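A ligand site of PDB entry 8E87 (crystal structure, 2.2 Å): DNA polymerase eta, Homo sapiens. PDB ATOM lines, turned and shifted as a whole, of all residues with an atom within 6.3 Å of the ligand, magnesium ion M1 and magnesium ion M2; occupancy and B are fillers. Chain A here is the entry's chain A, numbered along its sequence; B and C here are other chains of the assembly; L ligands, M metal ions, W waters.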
ATOM      1  N   ASP A  16       3.507  -3.896   0.095  1.00  0.00           N
ATOM      2  CA  ASP A  16       2.563  -3.274  -0.832  1.00  0.00           C
ATOM      3  C   ASP A  16       2.008  -4.303  -1.828  1.00  0.00           C
ATOM      4  O   ASP A  16       2.767  -4.975  -2.526  1.00  0.00           O
ATOM      5  CB  ASP A  16       3.268  -2.127  -1.573  1.00  0.00           C
ATOM      6  CG  ASP A  16       2.355  -1.366  -2.484  1.00  0.00           C
ATOM      7  OD1 ASP A  16       1.931  -1.911  -3.518  1.00  0.00           O
ATOM      8  OD2 ASP A  16       2.066  -0.201  -2.162  1.00  0.00           O
ATOM      9  N   MET A  17       0.677  -4.407  -1.887  1.00  0.00           N
ATOM     10  CA  MET A  17       0.052  -5.380  -2.775  1.00  0.00           C
ATOM     11  C   MET A  17       0.345  -5.057  -4.227  1.00  0.00           C
ATOM     12  O   MET A  17       0.351  -3.909  -4.643  1.00  0.00           O
ATOM     13  CB  MET A  17      -1.466  -5.465  -2.491  1.00  0.00           C
ATOM     14  CG  MET A  17      -1.754  -5.328  -1.002  1.00  0.00           C
ATOM     15  SD  MET A  17      -1.075  -6.751  -0.093  1.00  0.00           S
ATOM     16  CE  MET A  17      -1.642  -8.086  -1.150  1.00  0.00           C
ATOM     17  N   ASP A  18       0.659  -6.093  -4.994  1.00  0.00           N
ATOM     18  CA  ASP A  18       0.819  -5.957  -6.433  1.00  0.00           C
ATOM     19  C   ASP A  18      -0.540  -5.719  -7.109  1.00  0.00           C
ATOM     20  O   ASP A  18      -1.491  -6.466  -6.880  1.00  0.00           O
ATOM     21  CB  ASP A  18       1.471  -7.220  -6.997  1.00  0.00           C
ATOM     22  CG  ASP A  18       2.789  -7.539  -6.328  1.00  0.00           C
ATOM     23  OD1 ASP A  18       3.430  -6.594  -5.802  1.00  0.00           O
ATOM     24  OD2 ASP A  18       3.199  -8.709  -6.332  1.00  0.00           O
ATOM     25  N   CYS A  19      -0.584  -4.706  -7.976  1.00  0.00           N
ATOM     26  CA  CYS A  19      -1.771  -4.278  -8.715  1.00  0.00           C
ATOM     27  C   CYS A  19      -3.059  -4.583  -7.946  1.00  0.00           C
ATOM     28  O   CYS A  19      -3.883  -5.365  -8.424  1.00  0.00           O
ATOM     29  CB  CYS A  19      -1.787  -4.918 -10.114  1.00  0.00           C
ATOM     30  SG  CYS A  19      -1.764  -6.778 -10.250  1.00  0.00           S
ATOM     31  N   PHE A  20      -3.243  -3.948  -6.796  1.00  0.00           N
ATOM     32  CA  PHE A  20      -4.158  -4.443  -5.759  1.00  0.00           C
ATOM     33  C   PHE A  20      -5.617  -4.543  -6.232  1.00  0.00           C
ATOM     34  O   PHE A  20      -6.272  -5.587  -6.035  1.00  0.00           O
ATOM     35  CB  PHE A  20      -4.080  -3.520  -4.525  1.00  0.00           C
ATOM     36  CG  PHE A  20      -4.890  -4.004  -3.383  1.00  0.00           C
ATOM     37  CD1 PHE A  20      -4.857  -5.351  -3.018  1.00  0.00           C
ATOM     38  CD2 PHE A  20      -5.713  -3.128  -2.662  1.00  0.00           C
ATOM     39  CE1 PHE A  20      -5.616  -5.821  -1.954  1.00  0.00           C
ATOM     40  CE2 PHE A  20      -6.495  -3.613  -1.584  1.00  0.00           C
ATOM     41  CZ  PHE A  20      -6.432  -4.958  -1.241  1.00  0.00           C
ATOM     42  N   PHE A  21      -6.177  -3.458  -6.769  1.00  0.00           N
ATOM     43  CA  PHE A  21      -7.597  -3.563  -7.137  1.00  0.00           C
ATOM     44  C   PHE A  21      -7.804  -4.662  -8.188  1.00  0.00           C
ATOM     45  O   PHE A  21      -8.803  -5.397  -8.141  1.00  0.00           O
ATOM     46  CB  PHE A  21      -8.144  -2.210  -7.644  1.00  0.00           C
ATOM     47  CG  PHE A  21      -8.389  -1.166  -6.563  1.00  0.00           C
ATOM     48  CD1 PHE A  21      -7.768  -1.226  -5.346  1.00  0.00           C
ATOM     49  CD2 PHE A  21      -9.259  -0.120  -6.798  1.00  0.00           C
ATOM     50  CE1 PHE A  21      -8.002  -0.249  -4.349  1.00  0.00           C
ATOM     51  CE2 PHE A  21      -9.501   0.867  -5.834  1.00  0.00           C
ATOM     52  CZ  PHE A  21      -8.873   0.789  -4.595  1.00  0.00           C
ATOM     53  N   VAL A  22      -6.843  -4.827  -9.102  1.00  0.00           N
ATOM     54  CA  VAL A  22      -6.945  -5.868 -10.130  1.00  0.00           C
ATOM     55  C   VAL A  22      -6.921  -7.250  -9.498  1.00  0.00           C
ATOM     56  O   VAL A  22      -7.700  -8.139  -9.873  1.00  0.00           O
ATOM     57  CB  VAL A  22      -5.819  -5.705 -11.164  1.00  0.00           C
ATOM     58  CG1 VAL A  22      -5.734  -6.914 -12.051  1.00  0.00           C
ATOM     59  CG2 VAL A  22      -6.032  -4.470 -11.975  1.00  0.00           C
ATOM     60  N   GLN A  41     -12.809   3.350 -13.157  1.00  0.00           N
ATOM     61  CA  GLN A  41     -13.937   4.050 -12.536  1.00  0.00           C
ATOM     62  C   GLN A  41     -14.765   4.718 -13.636  1.00  0.00           C
ATOM     63  O   GLN A  41     -14.222   5.493 -14.434  1.00  0.00           O
ATOM     64  CB  GLN A  41     -13.446   5.095 -11.528  1.00  0.00           C
ATOM     65  CG  GLN A  41     -12.691   4.541 -10.329  1.00  0.00           C
ATOM     66  CD  GLN A  41     -12.356   5.588  -9.252  1.00  0.00           C
ATOM     67  OE1 GLN A  41     -12.715   5.417  -8.083  1.00  0.00           O
ATOM     68  NE2 GLN A  41     -11.677   6.669  -9.638  1.00  0.00           N
ATOM     69  N   ILE A  51      -7.276   2.960 -12.872  1.00  0.00           N
ATOM     70  CA  ILE A  51      -6.623   3.161 -11.579  1.00  0.00           C
ATOM     71  C   ILE A  51      -5.755   1.975 -11.133  1.00  0.00           C
ATOM     72  O   ILE A  51      -5.017   2.116 -10.142  1.00  0.00           O
ATOM     73  CB  ILE A  51      -7.629   3.522 -10.470  1.00  0.00           C
ATOM     74  CG1 ILE A  51      -8.706   2.461 -10.285  1.00  0.00           C
ATOM     75  CG2 ILE A  51      -8.310   4.900 -10.734  1.00  0.00           C
ATOM     76  CD1 ILE A  51      -9.617   2.671  -9.083  1.00  0.00           C
ATOM     77  N   ALA A  52      -5.777   0.821 -11.819  1.00  0.00           N
ATOM     78  CA  ALA A  52      -4.908  -0.302 -11.474  1.00  0.00           C
ATOM     79  C   ALA A  52      -4.713  -1.206 -12.699  1.00  0.00           C
ATOM     80  O   ALA A  52      -5.665  -1.431 -13.445  1.00  0.00           O
ATOM     81  CB  ALA A  52      -5.475  -1.136 -10.310  1.00  0.00           C
ATOM     82  N   VAL A  53      -3.499  -1.728 -12.877  1.00  0.00           N
ATOM     83  CA  VAL A  53      -3.104  -2.385 -14.122  1.00  0.00           C
ATOM     84  C   VAL A  53      -2.314  -3.640 -13.776  1.00  0.00           C
ATOM     85  O   VAL A  53      -1.323  -3.575 -13.048  1.00  0.00           O
ATOM     86  CB  VAL A  53      -2.267  -1.478 -15.034  1.00  0.00           C
ATOM     87  CG1 VAL A  53      -2.143  -2.084 -16.420  1.00  0.00           C
ATOM     88  CG2 VAL A  53      -2.857  -0.120 -15.116  1.00  0.00           C
ATOM     89  N   TYR A  55       0.330  -6.718 -14.408  1.00  0.00           N
ATOM     90  CA  TYR A  55       1.660  -6.614 -14.987  1.00  0.00           C
ATOM     91  C   TYR A  55       1.672  -7.104 -16.421  1.00  0.00           C
ATOM     92  O   TYR A  55       2.431  -6.578 -17.252  1.00  0.00           O
ATOM     93  CB  TYR A  55       2.651  -7.355 -14.072  1.00  0.00           C
ATOM     94  CG  TYR A  55       2.983  -6.489 -12.860  1.00  0.00           C
ATOM     95  CD1 TYR A  55       2.104  -6.393 -11.780  1.00  0.00           C
ATOM     96  CD2 TYR A  55       4.131  -5.707 -12.808  1.00  0.00           C
ATOM     97  CE1 TYR A  55       2.381  -5.595 -10.660  1.00  0.00           C
ATOM     98  CE2 TYR A  55       4.426  -4.903 -11.704  1.00  0.00           C
ATOM     99  CZ  TYR A  55       3.530  -4.844 -10.631  1.00  0.00           C
ATOM    100  OH  TYR A  55       3.791  -4.045  -9.538  1.00  0.00           O
ATOM    101  N   ARG A  58       0.623  -4.038 -18.198  1.00  0.00           N
ATOM    102  CA  ARG A  58       1.725  -3.086 -18.172  1.00  0.00           C
ATOM    103  C   ARG A  58       2.747  -3.365 -19.271  1.00  0.00           C
ATOM    104  O   ARG A  58       3.346  -2.423 -19.793  1.00  0.00           O
ATOM    105  CB  ARG A  58       2.418  -3.107 -16.805  1.00  0.00           C
ATOM    106  CG  ARG A  58       1.575  -2.570 -15.669  1.00  0.00           C
ATOM    107  CD  ARG A  58       2.324  -2.574 -14.348  1.00  0.00           C
ATOM    108  NE  ARG A  58       1.385  -2.445 -13.242  1.00  0.00           N
ATOM    109  CZ  ARG A  58       1.716  -2.131 -11.998  1.00  0.00           C
ATOM    110  NH1 ARG A  58       2.984  -1.944 -11.639  1.00  0.00           N
ATOM    111  NH2 ARG A  58       0.756  -1.989 -11.085  1.00  0.00           N
ATOM    112  N   ARG A  64      -1.864   3.572 -15.025  1.00  0.00           N
ATOM    113  CA  ARG A  64      -2.838   4.317 -14.251  1.00  0.00           C
ATOM    114  C   ARG A  64      -2.969   5.726 -14.820  1.00  0.00           C
ATOM    115  O   ARG A  64      -2.042   6.267 -15.433  1.00  0.00           O
ATOM    116  CB  ARG A  64      -2.412   4.352 -12.774  1.00  0.00           C
ATOM    117  CG  ARG A  64      -2.700   5.621 -12.007  1.00  0.00           C
ATOM    118  CD  ARG A  64      -1.998   5.633 -10.657  1.00  0.00           C
ATOM    119  NE  ARG A  64      -2.736   6.458  -9.704  1.00  0.00           N
ATOM    120  CZ  ARG A  64      -2.729   7.784  -9.703  1.00  0.00           C
ATOM    121  NH1 ARG A  64      -2.045   8.468 -10.600  1.00  0.00           N
ATOM    122  NH2 ARG A  64      -3.440   8.438  -8.792  1.00  0.00           N
ATOM    123  N   LEU A  92     -15.923   2.253  -3.184  1.00  0.00           N
ATOM    124  CA  LEU A  92     -14.696   1.471  -3.090  1.00  0.00           C
ATOM    125  C   LEU A  92     -14.731   0.466  -1.953  1.00  0.00           C
ATOM    126  O   LEU A  92     -13.677   0.025  -1.474  1.00  0.00           O
ATOM    127  CB  LEU A  92     -13.497   2.394  -2.963  1.00  0.00           C
ATOM    128  CG  LEU A  92     -13.340   3.419  -4.083  1.00  0.00           C
ATOM    129  CD1 LEU A  92     -12.169   4.339  -3.819  1.00  0.00           C
ATOM    130  CD2 LEU A  92     -13.181   2.707  -5.412  1.00  0.00           C
ATOM    131  N   SER A 116      -1.549   3.053   3.195  1.00  0.00           N
ATOM    132  CA  SER A 116      -2.562   3.288   2.174  1.00  0.00           C
ATOM    133  C   SER A 116      -3.453   2.063   2.133  1.00  0.00           C
ATOM    134  O   SER A 116      -3.140   1.048   2.778  1.00  0.00           O
ATOM    135  CB  SER A 116      -1.937   3.525   0.785  1.00  0.00           C
ATOM    136  OG  SER A 116      -1.593   2.290   0.173  1.00  0.00           O
ATOM    137  N   ILE A 117      -4.517   2.118   1.306  1.00  0.00           N
ATOM    138  CA  ILE A 117      -5.435   0.993   1.211  1.00  0.00           C
ATOM    139  C   ILE A 117      -4.702  -0.318   0.940  1.00  0.00           C
ATOM    140  O   ILE A 117      -5.161  -1.390   1.340  1.00  0.00           O
ATOM    141  CB  ILE A 117      -6.488   1.248   0.126  1.00  0.00           C
ATOM    142  CG1 ILE A 117      -7.667   0.302   0.307  1.00  0.00           C
ATOM    143  CG2 ILE A 117      -5.883   1.104  -1.269  1.00  0.00           C
ATOM    144  CD1 ILE A 117      -8.938   0.861  -0.387  1.00  0.00           C
ATOM    145  N   ASP A 118      -3.532  -0.250   0.290  1.00  0.00           N
ATOM    146  CA  ASP A 118      -2.844  -1.476  -0.083  1.00  0.00           C
ATOM    147  C   ASP A 118      -1.452  -1.610   0.493  1.00  0.00           C
ATOM    148  O   ASP A 118      -0.716  -2.516   0.079  1.00  0.00           O
ATOM    149  CB  ASP A 118      -2.787  -1.634  -1.611  1.00  0.00           C
ATOM    150  CG  ASP A 118      -1.529  -1.085  -2.239  1.00  0.00           C
ATOM    151  OD1 ASP A 118      -1.087   0.033  -1.848  1.00  0.00           O
ATOM    152  OD2 ASP A 118      -1.001  -1.764  -3.164  1.00  0.00           O
ATOM    153  N   GLU A 119      -1.053  -0.749   1.454  1.00  0.00           N
ATOM    154  CA  GLU A 119       0.296  -0.952   1.971  1.00  0.00           C
ATOM    155  C   GLU A 119       0.402  -0.556   3.436  1.00  0.00           C
ATOM    156  O   GLU A 119      -0.328   0.311   3.923  1.00  0.00           O
ATOM    157  CB  GLU A 119       1.355  -0.197   1.148  1.00  0.00           C
ATOM    158  CG  GLU A 119       1.427   1.275   1.396  1.00  0.00           C
ATOM    159  CD  GLU A 119       1.766   2.041   0.139  1.00  0.00           C
ATOM    160  OE1 GLU A 119       0.921   2.122  -0.768  1.00  0.00           O
ATOM    161  OE2 GLU A 119       2.922   2.513   0.040  1.00  0.00           O
ATOM    162  N   SER A 216       4.552  -7.326  -2.800  1.00  0.00           N
ATOM    163  CA  SER A 216       5.981  -7.141  -2.697  1.00  0.00           C
ATOM    164  C   SER A 216       6.307  -6.459  -1.381  1.00  0.00           C
ATOM    165  O   SER A 216       5.429  -5.955  -0.686  1.00  0.00           O
ATOM    166  CB  SER A 216       6.511  -6.343  -3.875  1.00  0.00           C
ATOM    167  OG  SER A 216       6.232  -7.011  -5.081  1.00  0.00           O
ATOM    168  N   LYS A 227      10.245   1.498   1.579  1.00  0.00           N
ATOM    169  CA  LYS A 227       9.340   1.810   0.478  1.00  0.00           C
ATOM    170  C   LYS A 227      10.089   1.823  -0.854  1.00  0.00           C
ATOM    171  O   LYS A 227       9.650   1.194  -1.825  1.00  0.00           O
ATOM    172  CB  LYS A 227       8.671   3.173   0.739  1.00  0.00           C
ATOM    173  CG  LYS A 227       7.814   3.731  -0.417  1.00  0.00           C
ATOM    174  CD  LYS A 227       6.542   2.906  -0.643  1.00  0.00           C
ATOM    175  CE  LYS A 227       5.643   3.505  -1.737  1.00  0.00           C
ATOM    176  NZ  LYS A 227       4.485   2.632  -2.047  1.00  0.00           N
ATOM    177  N   LYS A 234       9.236  -5.505  -7.832  1.00  0.00           N
ATOM    178  CA  LYS A 234       7.863  -5.887  -8.086  1.00  0.00           C
ATOM    179  C   LYS A 234       7.752  -6.558  -9.452  1.00  0.00           C
ATOM    180  O   LYS A 234       8.523  -6.234 -10.364  1.00  0.00           O
ATOM    181  CB  LYS A 234       6.997  -4.631  -8.026  1.00  0.00           C
ATOM    182  CG  LYS A 234       6.268  -4.436  -6.717  1.00  0.00           C
ATOM    183  CD  LYS A 234       5.448  -3.157  -6.652  1.00  0.00           C
ATOM    184  CE  LYS A 234       4.661  -3.071  -5.336  1.00  0.00           C
ATOM    185  NZ  LYS A 234       3.482  -4.029  -5.386  1.00  0.00           N
ATOM    186  N   PRO A 235       6.814  -7.499  -9.637  1.00  0.00           N
ATOM    187  CA  PRO A 235       5.850  -8.066  -8.681  1.00  0.00           C
ATOM    188  C   PRO A 235       6.327  -9.306  -7.958  1.00  0.00           C
ATOM    189  O   PRO A 235       7.250  -9.983  -8.378  1.00  0.00           O
ATOM    190  CB  PRO A 235       4.658  -8.418  -9.590  1.00  0.00           C
ATOM    191  CG  PRO A 235       5.340  -8.903 -10.845  1.00  0.00           C
ATOM    192  CD  PRO A 235       6.585  -8.038 -11.000  1.00  0.00           C
ATOM    193  P     A B   8       2.922   6.316  -4.132  1.00  0.00           P
ATOM    194  OP1   A B   8       3.910   5.203  -3.949  1.00  0.00           O
ATOM    195  OP2   A B   8       2.887   6.888  -5.522  1.00  0.00           O
ATOM    196  O5'   A B   8       1.470   5.733  -3.793  1.00  0.00           O
ATOM    197  C5'   A B   8       1.228   5.189  -2.474  1.00  0.00           C
ATOM    198  C4'   A B   8      -0.261   4.959  -2.315  1.00  0.00           C
ATOM    199  O4'   A B   8      -0.939   6.213  -2.522  1.00  0.00           O
ATOM    200  C3'   A B   8      -0.889   3.987  -3.318  1.00  0.00           C
ATOM    201  O3'   A B   8      -0.945   2.686  -2.748  1.00  0.00           O
ATOM    202  C2'   A B   8      -2.280   4.569  -3.609  1.00  0.00           C
ATOM    203  O2'   A B   8      -3.300   3.871  -2.948  1.00  0.00           O
ATOM    204  C1'   A B   8      -2.213   6.000  -3.082  1.00  0.00           C
ATOM    205  N9    A B   8      -2.438   7.051  -4.064  1.00  0.00           N
ATOM    206  C8    A B   8      -1.499   7.702  -4.814  1.00  0.00           C
ATOM    207  N7    A B   8      -2.001   8.646  -5.571  1.00  0.00           N
ATOM    208  C5    A B   8      -3.356   8.632  -5.287  1.00  0.00           C
ATOM    209  C6    A B   8      -4.435   9.408  -5.766  1.00  0.00           C
ATOM    210  N6    A B   8      -4.323  10.368  -6.673  1.00  0.00           N
ATOM    211  N1    A B   8      -5.659   9.135  -5.258  1.00  0.00           N
ATOM    212  C2    A B   8      -5.779   8.157  -4.355  1.00  0.00           C
ATOM    213  N3    A B   8      -4.839   7.381  -3.833  1.00  0.00           N
ATOM    214  C4    A B   8      -3.641   7.667  -4.348  1.00  0.00           C
ATOM    215  P    DT C   4     -11.314  13.658 -13.715  1.00  0.00           P
ATOM    216  OP1  DT C   4     -12.689  14.153 -14.058  1.00  0.00           O
ATOM    217  OP2  DT C   4     -10.439  14.649 -12.992  1.00  0.00           O
ATOM    218  O5'  DT C   4     -11.505  12.390 -12.755  1.00  0.00           O
ATOM    219  C5'  DT C   4     -12.434  11.360 -13.141  1.00  0.00           C
ATOM    220  C4'  DT C   4     -12.692  10.468 -11.950  1.00  0.00           C
ATOM    221  O4'  DT C   4     -11.445   9.890 -11.504  1.00  0.00           O
ATOM    222  C3'  DT C   4     -13.287  11.190 -10.740  1.00  0.00           C
ATOM    223  O3'  DT C   4     -14.234  10.322 -10.119  1.00  0.00           O
ATOM    224  C2'  DT C   4     -12.075  11.436  -9.852  1.00  0.00           C
ATOM    225  C1'  DT C   4     -11.222  10.217 -10.134  1.00  0.00           C
ATOM    226  N1   DT C   4      -9.775  10.441  -9.982  1.00  0.00           N
ATOM    227  C2   DT C   4      -9.064   9.561  -9.190  1.00  0.00           C
ATOM    228  O2   DT C   4      -9.585   8.627  -8.602  1.00  0.00           O
ATOM    229  N3   DT C   4      -7.727   9.826  -9.110  1.00  0.00           N
ATOM    230  C4   DT C   4      -7.048  10.851  -9.729  1.00  0.00           C
ATOM    231  O4   DT C   4      -5.834  10.966  -9.559  1.00  0.00           O
ATOM    232  C5   DT C   4      -7.844  11.730 -10.546  1.00  0.00           C
ATOM    233  C7   DT C   4      -7.178  12.874 -11.236  1.00  0.00           C
ATOM    234  C6   DT C   4      -9.162  11.479 -10.630  1.00  0.00           C
ATOM    235  P    DT C   5     -14.810  10.820  -8.718  1.00  0.00           P
ATOM    236  OP1  DT C   5     -16.207  10.330  -8.535  1.00  0.00           O
ATOM    237  OP2  DT C   5     -14.623  12.294  -8.466  1.00  0.00           O
ATOM    238  O5'  DT C   5     -13.891  10.031  -7.671  1.00  0.00           O
ATOM    239  C5'  DT C   5     -13.988   8.594  -7.632  1.00  0.00           C
ATOM    240  C4'  DT C   5     -13.318   8.081  -6.383  1.00  0.00           C
ATOM    241  O4'  DT C   5     -11.888   8.310  -6.455  1.00  0.00           O
ATOM    242  C3'  DT C   5     -13.797   8.734  -5.090  1.00  0.00           C
ATOM    243  O3'  DT C   5     -13.842   7.704  -4.094  1.00  0.00           O
ATOM    244  C2'  DT C   5     -12.712   9.745  -4.804  1.00  0.00           C
ATOM    245  C1'  DT C   5     -11.472   9.015  -5.299  1.00  0.00           C
ATOM    246  N1   DT C   5     -10.365   9.889  -5.694  1.00  0.00           N
ATOM    247  C2   DT C   5      -9.091   9.487  -5.356  1.00  0.00           C
ATOM    248  O2   DT C   5      -8.854   8.459  -4.756  1.00  0.00           O
ATOM    249  N3   DT C   5      -8.092  10.346  -5.763  1.00  0.00           N
ATOM    250  C4   DT C   5      -8.250  11.523  -6.457  1.00  0.00           C
ATOM    251  O4   DT C   5      -7.252  12.193  -6.749  1.00  0.00           O
ATOM    252  C5   DT C   5      -9.610  11.883  -6.770  1.00  0.00           C
ATOM    253  C7   DT C   5      -9.865  13.159  -7.519  1.00  0.00           C
ATOM    254  C6   DT C   5     -10.589  11.052  -6.387  1.00  0.00           C
ATOM    255  P    DT C   6     -14.496   7.975  -2.665  1.00  0.00           P
ATOM    256  OP1  DT C   6     -14.429   6.668  -2.005  1.00  0.00           O
ATOM    257  OP2  DT C   6     -15.801   8.650  -2.715  1.00  0.00           O
ATOM    258  O5'  DT C   6     -13.501   9.082  -2.077  1.00  0.00           O
ATOM    259  C5'  DT C   6     -12.956   8.938  -0.824  1.00  0.00           C
ATOM    260  C4'  DT C   6     -11.528   8.470  -0.924  1.00  0.00           C
ATOM    261  O4'  DT C   6     -10.801   9.287  -1.854  1.00  0.00           O
ATOM    262  C3'  DT C   6     -10.780   8.570   0.381  1.00  0.00           C
ATOM    263  O3'  DT C   6     -10.804   7.314   1.047  1.00  0.00           O
ATOM    264  C2'  DT C   6      -9.351   9.038  -0.002  1.00  0.00           C
ATOM    265  C1'  DT C   6      -9.442   9.235  -1.513  1.00  0.00           C
ATOM    266  N1   DT C   6      -8.758  10.466  -2.057  1.00  0.00           N
ATOM    267  C2   DT C   6      -7.402  10.443  -2.207  1.00  0.00           C
ATOM    268  O2   DT C   6      -6.713   9.513  -1.853  1.00  0.00           O
ATOM    269  N3   DT C   6      -6.873  11.552  -2.793  1.00  0.00           N
ATOM    270  C4   DT C   6      -7.558  12.666  -3.240  1.00  0.00           C
ATOM    271  O4   DT C   6      -6.986  13.630  -3.748  1.00  0.00           O
ATOM    272  C5   DT C   6      -8.976  12.625  -3.070  1.00  0.00           C
ATOM    273  C7   DT C   6      -9.836  13.776  -3.526  1.00  0.00           C
ATOM    274  C6   DT C   6      -9.511  11.520  -2.496  1.00  0.00           C
HETATM  275  N1  LIG L   1      -7.900   6.812  -7.414  1.00  0.00           N
HETATM  276  C1  LIG L   1      -8.443   5.722  -6.779  1.00  0.00           C
HETATM  277  N2  LIG L   1      -9.776   5.746  -6.632  1.00  0.00           N
HETATM  278  N3  LIG L   1      -7.779   4.645  -6.357  1.00  0.00           N
HETATM  279  C2  LIG L   1      -6.475   4.688  -6.612  1.00  0.00           C
HETATM  280  C3  LIG L   1      -5.810   5.693  -7.216  1.00  0.00           C
HETATM  281  C4  LIG L   1      -6.573   6.804  -7.634  1.00  0.00           C
HETATM  282  O1  LIG L   1      -6.063   7.774  -8.202  1.00  0.00           O
HETATM  283  N4  LIG L   1      -4.462   5.377  -7.331  1.00  0.00           N
HETATM  284  C5  LIG L   1      -4.357   4.189  -6.801  1.00  0.00           C
HETATM  285  N5  LIG L   1      -5.560   3.695  -6.361  1.00  0.00           N
HETATM  286  P1  LIG L   1      -0.661   1.280  -5.760  1.00  0.00           P
HETATM  287  P2  LIG L   1      -1.054  -1.085  -7.397  1.00  0.00           P
HETATM  288  P3  LIG L   1       1.641  -1.871  -7.700  1.00  0.00           P
HETATM  289  C6  LIG L   1      -5.843   2.336  -5.872  1.00  0.00           C
HETATM  290  O2  LIG L   1      -0.001   0.460  -4.750  1.00  0.00           O
HETATM  291  O3  LIG L   1      -1.257  -1.751  -6.114  1.00  0.00           O
HETATM  292  O4  LIG L   1       2.514  -1.010  -8.573  1.00  0.00           O
HETATM  293  C7  LIG L   1      -5.657   1.272  -6.941  1.00  0.00           C
HETATM  294  O5  LIG L   1       0.051   2.687  -5.951  1.00  0.00           O
HETATM  295  O6  LIG L   1      -2.323  -1.209  -8.316  1.00  0.00           O
HETATM  296  O7  LIG L   1       1.594  -1.482  -6.240  1.00  0.00           O
HETATM  297  C8  LIG L   1      -4.371   0.540  -6.544  1.00  0.00           C
HETATM  298  O8  LIG L   1      -4.517  -0.855  -6.841  1.00  0.00           O
HETATM  299  N6  LIG L   1      -0.723   0.510  -7.190  1.00  0.00           N
HETATM  300  O9  LIG L   1       0.133  -1.735  -8.185  1.00  0.00           O
HETATM  301  O10 LIG L   1       1.917  -3.360  -7.813  1.00  0.00           O
HETATM  302  C9  LIG L   1      -4.305   0.768  -5.038  1.00  0.00           C
HETATM  303  O11 LIG L   1      -4.949   2.048  -4.816  1.00  0.00           O
HETATM  304  C10 LIG L   1      -2.910   0.822  -4.461  1.00  0.00           C
HETATM  305  O12 LIG L   1      -2.100   1.680  -5.280  1.00  0.00           O
HETATM  306 MG    MG M   1       0.371  -1.694  -4.767  1.00  0.00          MG
HETATM  307 MG    MG M   2       0.551   1.146  -2.771  1.00  0.00          MG
HETATM  308  O   HOH W   1       2.030   2.204  -3.849  1.00  0.00           O
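Merely in contact with magnesium ion M2: Ser 116 (3.8 Å). Of the 27 residues printed, 5 come within 4 Å of magnesium ion M2.
Asp 18 touches the ligand (CA to O10, 3.1 Å). Ile 51 touches the ligand (O to C7, 3.4 Å). Ala 52 touches the ligand. CD1 of Leu 92 touches N2 of the ligand, 3.95 Å away. Ile 117 touches the ligand. Hydrophobic or aromatic side chains within 4 Å of the ligand: Phe 20, Phe 21, Ile 51, Ala 52, Tyr 55, Leu 92 and Ile 117. 19 residues have an atom within 4 Å of the ligand: Asp 16, Met 17, Asp 18, Cys 19, Phe 20, Phe 21, Gln 41, Ile 51, Ala 52, Tyr 55, Arg 58, Arg 64, Leu 92, Ile 117, Asp 118, Lys 234, A 8 of chain B, DT 4 of chain C and DT 5 of chain C.
Water W1 lies within hydrogen-bond range of O5 of the ligand (2.9 Å) and NZ of Lys 227 (3.1 Å).
NZ of Lys 227 sits close to OD2 of Asp 16 (3.7 Å). N of Asp 16 sits at hydrogen-bond distance from O of Ser 216, at 2.9 Å. The side-chain hydroxyl (OG) of Ser 116 lies close to the backbone NH (N) of Asp 118 (3.2 Å). OG of Ser 116 sits close to O3' of A 8 of chain B, 3.0 Å away. OP1 of A 8 of chain B lies within salt-bridge range of NZ of Lys 227. OH of Tyr 55 lies within hydrogen-bond range of NH1 of Arg 58 (3.1 Å). NZ of Lys 234 lies within salt-bridge range of OD1 of Asp 18, 2.6 Å away. The side-chain hydroxyl of Ser 216 sits at hydrogen-bond distance from the side-chain carboxylate of Asp 18 (2.9 Å).
NZ of Lys 234 touches magnesium ion M1, at 3.9 Å. Within 4 Å of magnesium ion M1: Asp 16, Met 17, Asp 118 and Lys 234. The nearest printed residue that does not touch magnesium ion M1 is Asp 18 (4.4 Å).
The side-chain hydroxyl (OH) of Tyr 55 lies within hydrogen-bond range of an oxygen (O10) of the ligand. O2 of DT 4 of chain C lies within hydrogen-bond range of N1 of the ligand, 2.7 Å away. An oxygen (O1) of the ligand sits at hydrogen-bond distance from the guanidinium group (NH2) of Arg 64, 2.8 Å away. O10 of the ligand is in hydrogen-bond range of N of Cys 19 (2.8 Å). The side-chain amino group (NZ) of Lys 234 is in salt-bridge range of an oxygen (O10) of the ligand, at 3.0 Å. O4 of the ligand lies within salt-bridge range of NH2 of Arg 58, 3.2 Å away. N of Phe 20 is in hydrogen-bond range of O6 of the ligand (3.3 Å). An oxygen (O8) of the ligand is in hydrogen-bond range of the backbone NH (N) of Phe 21 (3.1 Å). A nitrogen (N2) of the ligand lies within hydrogen-bond range of O4' of DT 5 of chain C (3.3 Å). O2 of DT 5 of chain C lies within hydrogen-bond range of a nitrogen (N1) of the ligand (3.3 Å). The side-chain amide oxygen (OE1) of Gln 41 lies within hydrogen-bond range of a nitrogen (N2) of the ligand (3.3 Å).
Magnesium ion M1 is bound by O7 of the ligand. OD1 of Asp 16 is bound to magnesium ion M1 (2.0 Å). Magnesium ion M1 is bound by OD2 of Asp 118 (2.1 Å). Magnesium ion M1 is bound by O3 of the ligand (2.1 Å). O2 of the ligand binds magnesium ion M1, 2.2 Å away. Magnesium ion M1 is bound by the backbone carbonyl oxygen (O) of Met 17 (2.2 Å). Magnesium ion M1 has six donor atoms within binding distance.
Magnesium ion M2 is bound by water W1, OD2 of Asp 16, O3' of A 8 of chain B, O2 of the ligand, OD1 of Asp 118 and OE1 of Glu 119. Magnesium ion M2 has six donor atoms within binding distance.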
